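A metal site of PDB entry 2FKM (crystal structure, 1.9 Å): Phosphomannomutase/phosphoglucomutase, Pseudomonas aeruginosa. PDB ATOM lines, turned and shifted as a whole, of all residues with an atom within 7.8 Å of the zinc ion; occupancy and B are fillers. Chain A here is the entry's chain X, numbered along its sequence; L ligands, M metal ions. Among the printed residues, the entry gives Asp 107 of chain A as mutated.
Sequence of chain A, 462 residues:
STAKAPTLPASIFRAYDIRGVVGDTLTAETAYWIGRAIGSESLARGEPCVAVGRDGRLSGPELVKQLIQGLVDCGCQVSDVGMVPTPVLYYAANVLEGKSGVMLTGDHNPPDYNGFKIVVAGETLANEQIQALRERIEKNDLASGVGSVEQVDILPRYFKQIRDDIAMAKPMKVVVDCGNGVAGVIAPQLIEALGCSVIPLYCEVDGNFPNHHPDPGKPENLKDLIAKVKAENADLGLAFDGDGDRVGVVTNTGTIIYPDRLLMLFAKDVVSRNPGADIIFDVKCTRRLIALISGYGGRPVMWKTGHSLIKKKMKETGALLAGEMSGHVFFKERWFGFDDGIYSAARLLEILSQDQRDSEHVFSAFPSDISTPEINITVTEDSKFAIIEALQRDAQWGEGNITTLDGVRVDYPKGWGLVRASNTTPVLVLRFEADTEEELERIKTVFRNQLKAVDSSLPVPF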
ATOM      1  N   ARG A  19     -11.600  -1.354  10.869  1.00  0.00           N
ATOM      2  CA  ARG A  19     -11.756  -2.376   9.825  1.00  0.00           C
ATOM      3  C   ARG A  19     -10.390  -2.760   9.292  1.00  0.00           C
ATOM      4  O   ARG A  19      -9.589  -1.893   8.968  1.00  0.00           O
ATOM      5  CB  ARG A  19     -12.640  -1.837   8.694  1.00  0.00           C
ATOM      6  CG  ARG A  19     -12.997  -2.820   7.565  1.00  0.00           C
ATOM      7  CD  ARG A  19     -14.049  -3.870   7.935  1.00  0.00           C
ATOM      8  NE  ARG A  19     -15.193  -3.353   8.691  1.00  0.00           N
ATOM      9  CZ  ARG A  19     -16.329  -2.871   8.174  1.00  0.00           C
ATOM     10  NH1 ARG A  19     -16.547  -2.815   6.862  1.00  0.00           N
ATOM     11  NH2 ARG A  19     -17.284  -2.446   8.991  1.00  0.00           N
ATOM     12  N   THR A  86     -25.409  -6.920  13.924  1.00  0.00           N
ATOM     13  CA  THR A  86     -24.960  -5.703  14.586  1.00  0.00           C
ATOM     14  C   THR A  86     -26.038  -4.971  15.374  1.00  0.00           C
ATOM     15  O   THR A  86     -25.802  -4.546  16.513  1.00  0.00           O
ATOM     16  CB  THR A  86     -24.332  -4.751  13.565  1.00  0.00           C
ATOM     17  OG1 THR A  86     -23.134  -5.344  13.066  1.00  0.00           O
ATOM     18  CG2 THR A  86     -23.997  -3.408  14.175  1.00  0.00           C
ATOM     19  N   PRO A  87     -27.238  -4.809  14.794  1.00  0.00           N
ATOM     20  CA  PRO A  87     -28.249  -4.169  15.594  1.00  0.00           C
ATOM     21  C   PRO A  87     -28.647  -4.943  16.871  1.00  0.00           C
ATOM     22  O   PRO A  87     -29.140  -4.345  17.821  1.00  0.00           O
ATOM     23  CB  PRO A  87     -29.429  -4.031  14.622  1.00  0.00           C
ATOM     24  CG  PRO A  87     -29.175  -4.989  13.535  1.00  0.00           C
ATOM     25  CD  PRO A  87     -27.694  -5.065  13.409  1.00  0.00           C
ATOM     26  N   THR A 105     -17.308  -7.228  13.541  1.00  0.00           N
ATOM     27  CA  THR A 105     -17.876  -7.416  12.221  1.00  0.00           C
ATOM     28  C   THR A 105     -17.025  -6.796  11.116  1.00  0.00           C
ATOM     29  O   THR A 105     -16.368  -5.780  11.321  1.00  0.00           O
ATOM     30  CB  THR A 105     -19.305  -6.842  12.134  1.00  0.00           C
ATOM     31  OG1 THR A 105     -19.828  -7.066  10.820  1.00  0.00           O
ATOM     32  CG2 THR A 105     -19.314  -5.364  12.432  1.00  0.00           C
ATOM     33  N   GLY A 106     -17.030  -7.455   9.958  1.00  0.00           N
ATOM     34  CA  GLY A 106     -16.493  -6.911   8.731  1.00  0.00           C
ATOM     35  C   GLY A 106     -17.595  -6.498   7.785  1.00  0.00           C
ATOM     36  O   GLY A 106     -17.324  -6.058   6.668  1.00  0.00           O
ATOM     37  N   ASP A 107     -18.833  -6.653   8.236  1.00  0.00           N
ATOM     38  CA  ASP A 107     -20.027  -6.186   7.540  1.00  0.00           C
ATOM     39  C   ASP A 107     -20.145  -6.868   6.171  1.00  0.00           C
ATOM     40  O   ASP A 107     -20.381  -8.078   6.151  1.00  0.00           O
ATOM     41  CB  ASP A 107     -20.046  -4.656   7.482  1.00  0.00           C
ATOM     42  CG  ASP A 107     -21.433  -4.109   7.232  1.00  0.00           C
ATOM     43  OD1 ASP A 107     -22.282  -4.854   6.693  1.00  0.00           O
ATOM     44  OD2 ASP A 107     -21.692  -2.930   7.584  1.00  0.00           O
ATOM     45  N   HIS A 108     -19.978  -6.142   5.060  1.00  0.00           N
ATOM     46  CA  HIS A 108     -20.050  -6.760   3.708  1.00  0.00           C
ATOM     47  C   HIS A 108     -18.764  -6.680   2.893  1.00  0.00           C
ATOM     48  O   HIS A 108     -18.781  -6.903   1.681  1.00  0.00           O
ATOM     49  CB  HIS A 108     -21.215  -6.186   2.892  1.00  0.00           C
ATOM     50  CG  HIS A 108     -21.161  -4.703   2.699  1.00  0.00           C
ATOM     51  ND1 HIS A 108     -21.869  -3.829   3.480  1.00  0.00           N
ATOM     52  CD2 HIS A 108     -20.499  -3.945   1.788  1.00  0.00           C
ATOM     53  CE1 HIS A 108     -21.642  -2.595   3.086  1.00  0.00           C
ATOM     54  NE2 HIS A 108     -20.809  -2.639   2.054  1.00  0.00           N
ATOM     55  N   LYS A 117     -17.351  -2.375  15.612  1.00  0.00           N
ATOM     56  CA  LYS A 117     -18.243  -1.252  15.790  1.00  0.00           C
ATOM     57  C   LYS A 117     -18.480  -1.109  17.270  1.00  0.00           C
ATOM     58  O   LYS A 117     -18.876  -2.081  17.932  1.00  0.00           O
ATOM     59  CB  LYS A 117     -19.543  -1.469  15.018  1.00  0.00           C
ATOM     60  CG  LYS A 117     -19.307  -1.364  13.492  1.00  0.00           C
ATOM     61  CD  LYS A 117     -20.588  -1.495  12.700  1.00  0.00           C
ATOM     62  CE  LYS A 117     -20.336  -1.832  11.249  1.00  0.00           C
ATOM     63  NZ  LYS A 117     -21.603  -2.076  10.491  1.00  0.00           N
ATOM     64  N   PRO A 214     -23.357  -9.688   0.576  1.00  0.00           N
ATOM     65  CA  PRO A 214     -24.553  -9.022   1.069  1.00  0.00           C
ATOM     66  C   PRO A 214     -24.425  -7.492   1.089  1.00  0.00           C
ATOM     67  O   PRO A 214     -24.252  -6.886   2.139  1.00  0.00           O
ATOM     68  CB  PRO A 214     -24.727  -9.609   2.474  1.00  0.00           C
ATOM     69  CG  PRO A 214     -23.366 -10.037   2.889  1.00  0.00           C
ATOM     70  CD  PRO A 214     -22.556 -10.293   1.668  1.00  0.00           C
ATOM     71  N   PRO A 216     -26.782  -4.613  -0.305  1.00  0.00           N
ATOM     72  CA  PRO A 216     -28.019  -4.178  -0.937  1.00  0.00           C
ATOM     73  C   PRO A 216     -27.934  -2.840  -1.672  1.00  0.00           C
ATOM     74  O   PRO A 216     -28.847  -2.517  -2.440  1.00  0.00           O
ATOM     75  CB  PRO A 216     -29.003  -4.049   0.237  1.00  0.00           C
ATOM     76  CG  PRO A 216     -28.370  -4.711   1.373  1.00  0.00           C
ATOM     77  CD  PRO A 216     -26.912  -4.674   1.166  1.00  0.00           C
ATOM     78  N   PHE A 240     -30.879  -7.757   3.245  1.00  0.00           N
ATOM     79  CA  PHE A 240     -30.093  -7.274   4.362  1.00  0.00           C
ATOM     80  C   PHE A 240     -28.630  -7.389   4.009  1.00  0.00           C
ATOM     81  O   PHE A 240     -28.233  -8.253   3.220  1.00  0.00           O
ATOM     82  CB  PHE A 240     -30.400  -8.085   5.627  1.00  0.00           C
ATOM     83  CG  PHE A 240     -31.821  -7.943   6.072  1.00  0.00           C
ATOM     84  CD1 PHE A 240     -32.236  -6.786   6.713  1.00  0.00           C
ATOM     85  CD2 PHE A 240     -32.743  -8.915   5.784  1.00  0.00           C
ATOM     86  CE1 PHE A 240     -33.550  -6.635   7.076  1.00  0.00           C
ATOM     87  CE2 PHE A 240     -34.057  -8.765   6.147  1.00  0.00           C
ATOM     88  CZ  PHE A 240     -34.450  -7.625   6.813  1.00  0.00           C
ATOM     89  N   ASP A 241     -27.838  -6.473   4.545  1.00  0.00           N
ATOM     90  CA  ASP A 241     -26.406  -6.521   4.270  1.00  0.00           C
ATOM     91  C   ASP A 241     -25.756  -7.478   5.255  1.00  0.00           C
ATOM     92  O   ASP A 241     -26.440  -8.141   6.030  1.00  0.00           O
ATOM     93  CB  ASP A 241     -25.799  -5.121   4.304  1.00  0.00           C
ATOM     94  CG  ASP A 241     -25.547  -4.612   5.699  1.00  0.00           C
ATOM     95  OD1 ASP A 241     -26.219  -5.036   6.643  1.00  0.00           O
ATOM     96  OD2 ASP A 241     -24.665  -3.756   5.834  1.00  0.00           O
ATOM     97  N   GLY A 242     -24.429  -7.571   5.217  1.00  0.00           N
ATOM     98  CA  GLY A 242     -23.696  -8.561   5.996  1.00  0.00           C
ATOM     99  C   GLY A 242     -24.031  -8.673   7.459  1.00  0.00           C
ATOM    100  O   GLY A 242     -24.224  -9.780   7.952  1.00  0.00           O
ATOM    101  N   ASP A 243     -24.077  -7.558   8.182  1.00  0.00           N
ATOM    102  CA  ASP A 243     -24.336  -7.611   9.627  1.00  0.00           C
ATOM    103  C   ASP A 243     -25.751  -7.172  10.028  1.00  0.00           C
ATOM    104  O   ASP A 243     -26.079  -7.179  11.215  1.00  0.00           O
ATOM    105  CB  ASP A 243     -23.255  -6.849  10.400  1.00  0.00           C
ATOM    106  CG  ASP A 243     -23.346  -5.333  10.254  1.00  0.00           C
ATOM    107  OD1 ASP A 243     -24.320  -4.819   9.666  1.00  0.00           O
ATOM    108  OD2 ASP A 243     -22.423  -4.667  10.747  1.00  0.00           O
ATOM    109  N   GLY A 244     -26.577  -6.788   9.054  1.00  0.00           N
ATOM    110  CA  GLY A 244     -27.994  -6.524   9.323  1.00  0.00           C
ATOM    111  C   GLY A 244     -28.370  -5.095   9.669  1.00  0.00           C
ATOM    112  O   GLY A 244     -29.541  -4.828   9.961  1.00  0.00           O
ATOM    113  N   ASP A 245     -27.424  -4.160   9.616  1.00  0.00           N
ATOM    114  CA  ASP A 245     -27.721  -2.728   9.869  1.00  0.00           C
ATOM    115  C   ASP A 245     -28.139  -1.903   8.652  1.00  0.00           C
ATOM    116  O   ASP A 245     -28.471  -0.724   8.811  1.00  0.00           O
ATOM    117  CB  ASP A 245     -26.592  -2.045  10.652  1.00  0.00           C
ATOM    118  CG  ASP A 245     -25.292  -1.969   9.894  1.00  0.00           C
ATOM    119  OD1 ASP A 245     -25.288  -2.212   8.674  1.00  0.00           O
ATOM    120  OD2 ASP A 245     -24.271  -1.660  10.515  1.00  0.00           O
ATOM    121  N   ARG A 246     -28.128  -2.506   7.467  1.00  0.00           N
ATOM    122  CA  ARG A 246     -28.689  -1.925   6.252  1.00  0.00           C
ATOM    123  C   ARG A 246     -29.827  -2.804   5.735  1.00  0.00           C
ATOM    124  O   ARG A 246     -29.779  -4.033   5.820  1.00  0.00           O
ATOM    125  CB  ARG A 246     -27.655  -1.808   5.112  1.00  0.00           C
ATOM    126  CG  ARG A 246     -26.463  -0.880   5.346  1.00  0.00           C
ATOM    127  CD  ARG A 246     -25.662  -0.725   4.046  1.00  0.00           C
ATOM    128  NE  ARG A 246     -24.343  -0.119   4.243  1.00  0.00           N
ATOM    129  CZ  ARG A 246     -23.588   0.395   3.279  1.00  0.00           C
ATOM    130  NH1 ARG A 246     -23.993   0.397   2.004  1.00  0.00           N
ATOM    131  NH2 ARG A 246     -22.405   0.908   3.575  1.00  0.00           N
ATOM    132  N   VAL A 247     -30.856  -2.160   5.189  1.00  0.00           N
ATOM    133  CA  VAL A 247     -31.919  -2.870   4.495  1.00  0.00           C
ATOM    134  C   VAL A 247     -32.071  -2.320   3.069  1.00  0.00           C
ATOM    135  O   VAL A 247     -31.877  -1.132   2.847  1.00  0.00           O
ATOM    136  CB  VAL A 247     -33.262  -2.765   5.245  1.00  0.00           C
ATOM    137  CG1 VAL A 247     -33.758  -1.323   5.311  1.00  0.00           C
ATOM    138  CG2 VAL A 247     -34.297  -3.666   4.606  1.00  0.00           C
ATOM    139  N   HIS A 307     -22.827   6.168   9.735  1.00  0.00           N
ATOM    140  CA  HIS A 307     -23.796   5.740  10.768  1.00  0.00           C
ATOM    141  C   HIS A 307     -23.465   6.239  12.175  1.00  0.00           C
ATOM    142  O   HIS A 307     -24.380   6.569  12.942  1.00  0.00           O
ATOM    143  CB  HIS A 307     -23.965   4.207  10.778  1.00  0.00           C
ATOM    144  CG  HIS A 307     -22.734   3.474  11.187  1.00  0.00           C
ATOM    145  ND1 HIS A 307     -22.541   3.004  12.472  1.00  0.00           N
ATOM    146  CD2 HIS A 307     -21.622   3.138  10.501  1.00  0.00           C
ATOM    147  CE1 HIS A 307     -21.365   2.413  12.553  1.00  0.00           C
ATOM    148  NE2 HIS A 307     -20.788   2.479  11.368  1.00  0.00           N
ATOM    149  N   SER A 326     -27.412   4.952   2.032  1.00  0.00           N
ATOM    150  CA  SER A 326     -26.826   3.623   1.930  1.00  0.00           C
ATOM    151  C   SER A 326     -27.675   2.551   2.582  1.00  0.00           C
ATOM    152  O   SER A 326     -27.404   1.369   2.414  1.00  0.00           O
ATOM    153  CB  SER A 326     -25.446   3.602   2.583  1.00  0.00           C
ATOM    154  OG  SER A 326     -25.566   4.037   3.914  1.00  0.00           O
ATOM    155  N   HIS A 328     -28.883   2.522   6.084  1.00  0.00           N
ATOM    156  CA  HIS A 328     -28.995   2.546   7.536  1.00  0.00           C
ATOM    157  C   HIS A 328     -30.155   3.451   7.918  1.00  0.00           C
ATOM    158  O   HIS A 328     -30.147   4.625   7.562  1.00  0.00           O
ATOM    159  CB  HIS A 328     -27.734   3.121   8.156  1.00  0.00           C
ATOM    160  CG  HIS A 328     -26.495   2.302   7.954  1.00  0.00           C
ATOM    161  ND1 HIS A 328     -25.771   2.330   6.785  1.00  0.00           N
ATOM    162  CD2 HIS A 328     -25.825   1.479   8.791  1.00  0.00           C
ATOM    163  CE1 HIS A 328     -24.721   1.536   6.903  1.00  0.00           C
ATOM    164  NE2 HIS A 328     -24.726   1.019   8.118  1.00  0.00           N
ATOM    165  N   ASP A 339     -29.240   2.180  14.248  1.00  0.00           N
ATOM    166  CA  ASP A 339     -29.573   1.682  12.926  1.00  0.00           C
ATOM    167  C   ASP A 339     -29.805   0.172  12.953  1.00  0.00           C
ATOM    168  O   ASP A 339     -29.084  -0.582  13.606  1.00  0.00           O
ATOM    169  CB  ASP A 339     -28.484   2.015  11.899  1.00  0.00           C
ATOM    170  CG  ASP A 339     -27.061   1.881  12.447  1.00  0.00           C
ATOM    171  OD1 ASP A 339     -26.841   2.108  13.647  1.00  0.00           O
ATOM    172  OD2 ASP A 339     -26.151   1.591  11.644  1.00  0.00           O
HETATM  173  C1  LIG L   1     -20.992   3.303   6.242  1.00  0.00           C
HETATM  174  C2  LIG L   1     -21.951   4.501   6.213  1.00  0.00           C
HETATM  175  C3  LIG L   1     -22.697   4.597   4.896  1.00  0.00           C
HETATM  176  C4  LIG L   1     -21.669   4.927   3.861  1.00  0.00           C
HETATM  177  C5  LIG L   1     -20.606   3.825   3.835  1.00  0.00           C
HETATM  178  C6  LIG L   1     -19.242   4.459   3.849  1.00  0.00           C
HETATM  179  O1  LIG L   1     -21.601   2.203   6.919  1.00  0.00           O
HETATM  180  O2  LIG L   1     -22.884   4.424   7.275  1.00  0.00           O
HETATM  181  O3  LIG L   1     -23.653   5.644   4.848  1.00  0.00           O
HETATM  182  O4  LIG L   1     -22.252   5.122   2.582  1.00  0.00           O
HETATM  183  O5  LIG L   1     -20.652   2.888   4.919  1.00  0.00           O
HETATM  184  O6  LIG L   1     -19.437   5.862   3.786  1.00  0.00           O
HETATM  185  P1  LIG L   1     -18.649   6.698   2.844  1.00  0.00           P
HETATM  186  O7  LIG L   1     -18.029   7.793   3.651  1.00  0.00           O
HETATM  187  O8  LIG L   1     -19.558   7.239   1.802  1.00  0.00           O
HETATM  188  O9  LIG L   1     -17.572   5.855   2.226  1.00  0.00           O
HETATM  189  P2  LIG L   1     -20.885   0.988   7.477  1.00  0.00           P
HETATM  190  O10 LIG L   1     -20.936  -0.165   6.513  1.00  0.00           O
HETATM  191  O11 LIG L   1     -21.599   0.558   8.727  1.00  0.00           O
HETATM  192  O12 LIG L   1     -19.441   1.283   7.809  1.00  0.00           O
HETATM  193 ZN    ZN M   1     -23.846  -3.038   7.574  1.00  0.00          ZN
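OD1 of Asp 241 is in hydrogen-bond range of N of Arg 246 (3.3 Å). The backbone NH (N) of Gly 244 sits at hydrogen-bond distance from the side-chain carboxylate (OD1) of Asp 241 (3.0 Å). OG1 of Thr 105 lies within hydrogen-bond range of N of Asp 107 (2.8 Å). NE2 of His 328 sits close to OD1 of Asp 245, 3.3 Å away. The side-chain carboxylate (OD2) of Asp 243 is in salt-bridge range of the side-chain amino group (NZ) of Lys 117 (2.7 Å). OG1 of Thr 86 is in hydrogen-bond range of OD2 of Asp 243 (2.5 Å). The side-chain carboxylate of Asp 107 lies close to the side-chain amino group of Lys 117, at 3.0 Å. The side-chain carboxylate (OD2) of Asp 245 lies within salt-bridge range of the side-chain amino group (NZ) of Lys 117, at 2.7 Å.
Lys 117 touches the zinc ion (NZ to ZN, 3.8 Å). Within 4 Å of the zinc ion: Asp 107, Lys 117, Asp 241, Asp 243 and Asp 245. The nearest printed residue that does not touch the zinc ion is Arg 246 (4.1 Å).
OD1 of Asp 245 is bound to the zinc ion (2.0 Å). The zinc ion is bound by the side-chain carboxylate (OD2) of Asp 241. The zinc ion is bound by OD2 of Asp 107 (2.2 Å). The side-chain carboxylate (OD1) of Asp 107 is bound to the zinc ion, 2.6 Å away. Slightly farther from the zinc ion lies OD1 of Asp 243 (2.8 Å).
N of His 307 is in hydrogen-bond range of O2 of the ligand (3.0 Å). An oxygen (O10) of the ligand lies within salt-bridge range of the guanidinium group of Arg 246, 3.5 Å away. An oxygen (O3) of the ligand lies within hydrogen-bond range of the side-chain hydroxyl of Ser 326, at 2.7 Å. O10 of the ligand lies close to OD2 of Asp 107. An oxygen (O11) of the ligand sits close to a ring nitrogen (NE2) of His 307 (3.4 Å). A ring nitrogen (NE2) of His 328 sits at hydrogen-bond distance from an oxygen (O11) of the ligand (3.2 Å). NZ of Lys 117 lies within salt-bridge range of O11 of the ligand, at 3.2 Å.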
